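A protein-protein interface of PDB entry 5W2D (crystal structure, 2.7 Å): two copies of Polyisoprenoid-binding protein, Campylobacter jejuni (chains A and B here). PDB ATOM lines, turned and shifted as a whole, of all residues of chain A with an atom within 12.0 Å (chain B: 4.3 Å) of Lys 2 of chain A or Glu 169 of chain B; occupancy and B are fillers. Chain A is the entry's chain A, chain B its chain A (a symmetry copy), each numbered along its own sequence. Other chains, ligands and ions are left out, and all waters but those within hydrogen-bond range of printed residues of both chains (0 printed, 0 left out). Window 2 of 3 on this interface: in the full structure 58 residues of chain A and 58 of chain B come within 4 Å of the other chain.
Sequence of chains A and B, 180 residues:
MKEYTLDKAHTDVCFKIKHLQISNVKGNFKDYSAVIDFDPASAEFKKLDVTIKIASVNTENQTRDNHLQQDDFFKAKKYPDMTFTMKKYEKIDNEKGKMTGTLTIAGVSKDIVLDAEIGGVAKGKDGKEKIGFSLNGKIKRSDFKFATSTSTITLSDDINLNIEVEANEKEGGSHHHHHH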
ATOM      1  N   MET A   1     -16.888 -36.672  -3.824  1.00  0.00           N
ATOM      2  CA  MET A   1     -17.381 -35.353  -4.329  1.00  0.00           C
ATOM      3  C   MET A   1     -17.273 -34.179  -3.311  1.00  0.00           C
ATOM      4  O   MET A   1     -16.325 -34.108  -2.557  1.00  0.00           O
ATOM      5  CB  MET A   1     -18.772 -35.493  -4.995  1.00  0.00           C
ATOM      6  CG  MET A   1     -19.859 -36.208  -4.206  1.00  0.00           C
ATOM      7  SD  MET A   1     -20.437 -35.301  -2.744  1.00  0.00           S
ATOM      8  CE  MET A   1     -19.938 -36.442  -1.428  1.00  0.00           C
ATOM      9  N   LYS A   2     -18.222 -33.252  -3.331  1.00  0.00           N
ATOM     10  CA  LYS A   2     -18.212 -32.063  -2.487  1.00  0.00           C
ATOM     11  C   LYS A   2     -19.572 -31.401  -2.569  1.00  0.00           C
ATOM     12  O   LYS A   2     -20.283 -31.544  -3.574  1.00  0.00           O
ATOM     13  CB  LYS A   2     -17.109 -31.073  -2.883  1.00  0.00           C
ATOM     14  CG  LYS A   2     -15.975 -31.089  -1.892  1.00  0.00           C
ATOM     15  CD  LYS A   2     -14.722 -30.346  -2.310  1.00  0.00           C
ATOM     16  CE  LYS A   2     -13.607 -30.736  -1.337  1.00  0.00           C
ATOM     17  NZ  LYS A   2     -12.720 -29.571  -0.983  1.00  0.00           N
ATOM     18  N   GLU A   3     -19.926 -30.681  -1.506  1.00  0.00           N
ATOM     19  CA  GLU A   3     -21.236 -30.044  -1.392  1.00  0.00           C
ATOM     20  C   GLU A   3     -21.130 -28.530  -1.365  1.00  0.00           C
ATOM     21  O   GLU A   3     -20.197 -27.955  -0.784  1.00  0.00           O
ATOM     22  CB  GLU A   3     -21.975 -30.526  -0.155  1.00  0.00           C
ATOM     23  CG  GLU A   3     -22.474 -31.954  -0.242  1.00  0.00           C
ATOM     24  CD  GLU A   3     -22.847 -32.498   1.120  1.00  0.00           C
ATOM     25  OE1 GLU A   3     -22.481 -33.656   1.421  1.00  0.00           O
ATOM     26  OE2 GLU A   3     -23.490 -31.756   1.895  1.00  0.00           O
ATOM     27  N   TYR A   4     -22.091 -27.892  -2.023  1.00  0.00           N
ATOM     28  CA  TYR A   4     -22.075 -26.445  -2.151  1.00  0.00           C
ATOM     29  C   TYR A   4     -23.438 -25.898  -1.767  1.00  0.00           C
ATOM     30  O   TYR A   4     -24.447 -26.612  -1.815  1.00  0.00           O
ATOM     31  CB  TYR A   4     -21.658 -26.022  -3.574  1.00  0.00           C
ATOM     32  CG  TYR A   4     -20.290 -26.548  -3.996  1.00  0.00           C
ATOM     33  CD1 TYR A   4     -20.093 -27.928  -4.327  1.00  0.00           C
ATOM     34  CD2 TYR A   4     -19.196 -25.676  -4.091  1.00  0.00           C
ATOM     35  CE1 TYR A   4     -18.842 -28.409  -4.703  1.00  0.00           C
ATOM     36  CE2 TYR A   4     -17.939 -26.148  -4.479  1.00  0.00           C
ATOM     37  CZ  TYR A   4     -17.764 -27.507  -4.780  1.00  0.00           C
ATOM     38  OH  TYR A   4     -16.510 -27.950  -5.158  1.00  0.00           O
ATOM     39  N   THR A   5     -23.437 -24.642  -1.351  1.00  0.00           N
ATOM     40  CA  THR A   5     -24.638 -23.917  -1.007  1.00  0.00           C
ATOM     41  C   THR A   5     -24.615 -22.795  -1.989  1.00  0.00           C
ATOM     42  O   THR A   5     -23.547 -22.210  -2.179  1.00  0.00           O
ATOM     43  CB  THR A   5     -24.506 -23.320   0.417  1.00  0.00           C
ATOM     44  OG1 THR A   5     -24.290 -24.378   1.364  1.00  0.00           O
ATOM     45  CG2 THR A   5     -25.751 -22.479   0.828  1.00  0.00           C
ATOM     46  N   LEU A   6     -25.756 -22.459  -2.595  1.00  0.00           N
ATOM     47  CA  LEU A   6     -25.824 -21.233  -3.437  1.00  0.00           C
ATOM     48  C   LEU A   6     -25.355 -19.980  -2.686  1.00  0.00           C
ATOM     49  O   LEU A   6     -25.344 -19.947  -1.454  1.00  0.00           O
ATOM     50  CB  LEU A   6     -27.230 -20.981  -3.998  1.00  0.00           C
ATOM     51  CG  LEU A   6     -27.943 -22.083  -4.778  1.00  0.00           C
ATOM     52  CD1 LEU A   6     -28.697 -23.070  -3.882  1.00  0.00           C
ATOM     53  CD2 LEU A   6     -28.904 -21.370  -5.693  1.00  0.00           C
ATOM     54  N   ASP A   7     -24.911 -18.985  -3.436  1.00  0.00           N
ATOM     55  CA  ASP A   7     -24.798 -17.633  -2.939  1.00  0.00           C
ATOM     56  C   ASP A   7     -25.844 -16.882  -3.758  1.00  0.00           C
ATOM     57  O   ASP A   7     -25.589 -16.499  -4.904  1.00  0.00           O
ATOM     58  CB  ASP A   7     -23.366 -17.083  -3.120  1.00  0.00           C
ATOM     59  CG  ASP A   7     -23.290 -15.533  -3.095  1.00  0.00           C
ATOM     60  OD1 ASP A   7     -24.184 -14.858  -2.527  1.00  0.00           O
ATOM     61  OD2 ASP A   7     -22.312 -14.981  -3.650  1.00  0.00           O
ATOM     62  N   LYS A   8     -27.029 -16.706  -3.168  1.00  0.00           N
ATOM     63  CA  LYS A   8     -28.180 -16.070  -3.832  1.00  0.00           C
ATOM     64  C   LYS A   8     -27.890 -14.668  -4.422  1.00  0.00           C
ATOM     65  O   LYS A   8     -28.545 -14.264  -5.403  1.00  0.00           O
ATOM     66  CB  LYS A   8     -29.412 -16.033  -2.907  1.00  0.00           C
ATOM     67  CG  LYS A   8     -30.112 -17.372  -2.665  1.00  0.00           C
ATOM     68  CD  LYS A   8     -31.637 -17.200  -2.635  1.00  0.00           C
ATOM     69  CE  LYS A   8     -32.356 -18.184  -1.714  1.00  0.00           C
ATOM     70  NZ  LYS A   8     -31.826 -19.577  -1.803  1.00  0.00           N
ATOM     71  N   THR A  11     -26.420 -15.310  -7.995  1.00  0.00           N
ATOM     72  CA  THR A  11     -27.132 -16.417  -8.664  1.00  0.00           C
ATOM     73  C   THR A  11     -28.455 -15.884  -9.230  1.00  0.00           C
ATOM     74  O   THR A  11     -29.156 -15.099  -8.571  1.00  0.00           O
ATOM     75  CB  THR A  11     -27.351 -17.636  -7.726  1.00  0.00           C
ATOM     76  OG1 THR A  11     -26.108 -18.315  -7.513  1.00  0.00           O
ATOM     77  CG2 THR A  11     -28.327 -18.637  -8.306  1.00  0.00           C
ATOM     78  N   ILE B  36     -26.447 -28.853  -4.304  1.00  0.00           N
ATOM     79  CA  ILE B  36     -25.375 -28.933  -5.302  1.00  0.00           C
ATOM     80  C   ILE B  36     -24.216 -29.881  -4.889  1.00  0.00           C
ATOM     81  O   ILE B  36     -23.426 -29.573  -3.986  1.00  0.00           O
ATOM     82  CB  ILE B  36     -24.839 -27.524  -5.645  1.00  0.00           C
ATOM     83  CG1 ILE B  36     -25.994 -26.539  -5.913  1.00  0.00           C
ATOM     84  CG2 ILE B  36     -23.896 -27.617  -6.829  1.00  0.00           C
ATOM     85  CD1 ILE B  36     -25.627 -25.063  -5.930  1.00  0.00           C
ATOM     86  N   ASP B  37     -24.133 -31.025  -5.571  1.00  0.00           N
ATOM     87  CA  ASP B  37     -23.056 -31.998  -5.378  1.00  0.00           C
ATOM     88  C   ASP B  37     -22.126 -32.071  -6.563  1.00  0.00           C
ATOM     89  O   ASP B  37     -22.519 -32.581  -7.628  1.00  0.00           O
ATOM     90  CB  ASP B  37     -23.626 -33.381  -5.211  1.00  0.00           C
ATOM     91  CG  ASP B  37     -23.937 -33.713  -3.795  1.00  0.00           C
ATOM     92  OD1 ASP B  37     -23.945 -32.771  -2.944  1.00  0.00           O
ATOM     93  OD2 ASP B  37     -24.183 -34.934  -3.565  1.00  0.00           O
ATOM     94  N   PHE B  38     -20.887 -31.617  -6.362  1.00  0.00           N
ATOM     95  CA  PHE B  38     -19.948 -31.435  -7.469  1.00  0.00           C
ATOM     96  C   PHE B  38     -18.503 -31.778  -7.129  1.00  0.00           C
ATOM     97  O   PHE B  38     -17.964 -31.270  -6.154  1.00  0.00           O
ATOM     98  CB  PHE B  38     -20.030 -29.996  -8.005  1.00  0.00           C
ATOM     99  CG  PHE B  38     -19.143 -29.749  -9.182  1.00  0.00           C
ATOM    100  CD1 PHE B  38     -19.513 -30.199 -10.453  1.00  0.00           C
ATOM    101  CD2 PHE B  38     -17.910 -29.096  -9.017  1.00  0.00           C
ATOM    102  CE1 PHE B  38     -18.669 -29.986 -11.539  1.00  0.00           C
ATOM    103  CE2 PHE B  38     -17.063 -28.881 -10.099  1.00  0.00           C
ATOM    104  CZ  PHE B  38     -17.446 -29.319 -11.366  1.00  0.00           C
ATOM    105  N   LYS B 128     -11.683 -21.917   1.777  1.00  0.00           N
ATOM    106  CA  LYS B 128     -12.824 -22.770   1.405  1.00  0.00           C
ATOM    107  C   LYS B 128     -13.278 -22.552  -0.043  1.00  0.00           C
ATOM    108  O   LYS B 128     -13.276 -21.421  -0.550  1.00  0.00           O
ATOM    109  CB  LYS B 128     -13.996 -22.604   2.391  1.00  0.00           C
ATOM    110  CG  LYS B 128     -13.966 -23.626   3.526  1.00  0.00           C
ATOM    111  CD  LYS B 128     -15.167 -23.556   4.477  1.00  0.00           C
ATOM    112  CE  LYS B 128     -15.223 -24.795   5.352  1.00  0.00           C
ATOM    113  NZ  LYS B 128     -16.071 -24.550   6.610  1.00  0.00           N
ATOM    114  N   GLU B 129     -13.670 -23.661  -0.674  1.00  0.00           N
ATOM    115  CA  GLU B 129     -14.078 -23.756  -2.092  1.00  0.00           C
ATOM    116  C   GLU B 129     -15.239 -22.867  -2.605  1.00  0.00           C
ATOM    117  O   GLU B 129     -16.231 -22.617  -1.908  1.00  0.00           O
ATOM    118  CB  GLU B 129     -14.461 -25.212  -2.393  1.00  0.00           C
ATOM    119  CG  GLU B 129     -13.303 -26.191  -2.516  1.00  0.00           C
ATOM    120  CD  GLU B 129     -13.013 -26.622  -3.948  1.00  0.00           C
ATOM    121  OE1 GLU B 129     -12.003 -27.327  -4.122  1.00  0.00           O
ATOM    122  OE2 GLU B 129     -13.770 -26.277  -4.897  1.00  0.00           O
ATOM    123  N   ASN B 168     -20.734 -21.839  -2.804  1.00  0.00           N
ATOM    124  CA  ASN B 168     -19.660 -22.086  -1.846  1.00  0.00           C
ATOM    125  C   ASN B 168     -19.826 -23.450  -1.193  1.00  0.00           C
ATOM    126  O   ASN B 168     -20.934 -23.983  -1.110  1.00  0.00           O
ATOM    127  CB  ASN B 168     -19.594 -20.944  -0.830  1.00  0.00           C
ATOM    128  CG  ASN B 168     -19.343 -19.599  -1.500  1.00  0.00           C
ATOM    129  OD1 ASN B 168     -18.207 -19.271  -1.863  1.00  0.00           O
ATOM    130  ND2 ASN B 168     -20.414 -18.826  -1.710  1.00  0.00           N
ATOM    131  N   GLU B 169     -18.698 -24.020  -0.771  1.00  0.00           N
ATOM    132  CA  GLU B 169     -18.644 -25.335  -0.129  1.00  0.00           C
ATOM    133  C   GLU B 169     -19.435 -25.313   1.207  1.00  0.00           C
ATOM    134  O   GLU B 169     -19.669 -24.233   1.783  1.00  0.00           O
ATOM    135  CB  GLU B 169     -17.173 -25.695   0.091  1.00  0.00           C
ATOM    136  CG  GLU B 169     -16.829 -27.181   0.096  1.00  0.00           C
ATOM    137  CD  GLU B 169     -15.405 -27.469   0.607  1.00  0.00           C
ATOM    138  OE1 GLU B 169     -15.080 -28.669   0.790  1.00  0.00           O
ATOM    139  OE2 GLU B 169     -14.604 -26.516   0.833  1.00  0.00           O
ATOM    140  N   LYS B 170     -19.844 -26.486   1.700  1.00  0.00           N
ATOM    141  CA  LYS B 170     -20.748 -26.558   2.856  1.00  0.00           C
ATOM    142  C   LYS B 170     -20.084 -26.511   4.251  1.00  0.00           C
ATOM    143  O   LYS B 170     -18.909 -26.887   4.403  1.00  0.00           O
ATOM    144  CB  LYS B 170     -21.706 -27.751   2.729  1.00  0.00           C
ATOM    145  CG  LYS B 170     -23.170 -27.340   2.858  1.00  0.00           C
ATOM    146  CD  LYS B 170     -24.067 -28.503   3.246  1.00  0.00           C
ATOM    147  CE  LYS B 170     -25.311 -27.950   3.968  1.00  0.00           C
ATOM    148  NZ  LYS B 170     -26.254 -29.030   4.410  1.00  0.00           N
ATOM    149  N   GLU B 171     -20.862 -26.048   5.249  1.00  0.00           N
ATOM    150  CA  GLU B 171     -20.494 -25.986   6.689  1.00  0.00           C
ATOM    151  C   GLU B 171     -19.245 -25.140   6.967  1.00  0.00           C
ATOM    152  O   GLU B 171     -19.174 -23.973   6.571  1.00  0.00           O
ATOM    153  CB  GLU B 171     -20.385 -27.392   7.328  1.00  0.00           C
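O of Ile 36 of chain B lies within hydrogen-bond range of N of Tyr 4 of chain A (2.9 Å).
The side-chain carboxylate of Glu 129 of chain B is in hydrogen-bond range of the side-chain hydroxyl of Tyr 4 of chain A (3.2 Å).
NZ of Lys 2 of chain A lies within salt-bridge range of OE1 of Glu 129 of chain B, at 3.9 Å.
N of Thr 5 of chain A lies within hydrogen-bond range of O of Asn 168 of chain B.
O of Glu 3 of chain A is in hydrogen-bond range of N of Lys 170 of chain B (2.9 Å).
The side-chain amino group of Lys 2 of chain A is in salt-bridge range of the side-chain carboxylate of Glu 169 of chain B, at 3.1 Å.
N of Phe 38 of chain B lies within hydrogen-bond range of O of Lys 2 of chain A.
N of Glu 169 of chain B is in hydrogen-bond range of O of Glu 129 of chain B.
OG1 of Thr 11 of chain A lies within hydrogen-bond range of O of Asp 7 of chain A.
Met 1 of chain A touches Asp 37 of chain B.
Lys 2 of chain A touches Ile 36 of chain B.
Lys 2 of chain A touches Asp 37 of chain B.
Glu 3 of chain A touches Glu 169 of chain B (O to CA, 3.1 Å).
Tyr 4 of chain A touches Phe 38 of chain B (CE1 to O, 3.3 Å).
Tyr 4 of chain A touches Asn 168 of chain B.
CD2 of Tyr 4 of chain A touches N of Glu 169 of chain B (3.7 Å).
Lys 170 of chain B touches Thr 5 of chain A (CG to OG1, 3.5 Å).
CG of Leu 6 of chain A touches CD1 of Ile 36 of chain B, 3.9 Å away.
CB of Asp 7 of chain A touches ND2 of Asn 168 of chain B (3.7 Å).
Of the printed residues of chain B, Met 1 of chain A touches Asp 37 (3.9 Å).
Lys 2 of chain A touches five residues of chain B.
Of the printed residues of chain B, Tyr 4 of chain A touches Ile 36 (2.9 Å), Phe 38 (3.3 Å), Glu 129 (3.2 Å), Asn 168 (2.9 Å) and Glu 169 (3.7 Å).
Of the printed residues of chain B, Leu 6 of chain A touches Ile 36 (3.9 Å).
Lys 8 of chain A touches none of the printed residues of chain B.
Thr 11 of chain A touches none of the printed residues of chain B.
Of the printed residues of chain A, Asp 37 of chain B touches Met 1, Lys 2 and Glu 3.
Glu 129 of chain B touches just these residues of chain A: Lys 2 and Tyr 4.
Asn 168 of chain B touches just these residues of chain A: Tyr 4 (2.9 Å), Thr 5 (2.6 Å) and Asp 7 (3.7 Å).
Glu 169 of chain B touches just these residues of chain A: Lys 2 (3.1 Å), Glu 3 (3.1 Å) and Tyr 4 (3.7 Å).
Of the printed residues of chain A, Lys 170 of chain B touches Glu 3 (2.9 Å) and Thr 5 (3.5 Å).
No residue of chain A comes within 4 Å of Glu 171 of chain B.
The nearest printed residue of chain B that does not touch Lys 2 of chain A is Lys 170 of chain B (6.5 Å).
Of the 9 printed residues of chain B, 7 touch a printed residue of chain A.
Of the 9 printed residues of chain A, 7 touch a printed residue of chain B.
No position is printed for both chains.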
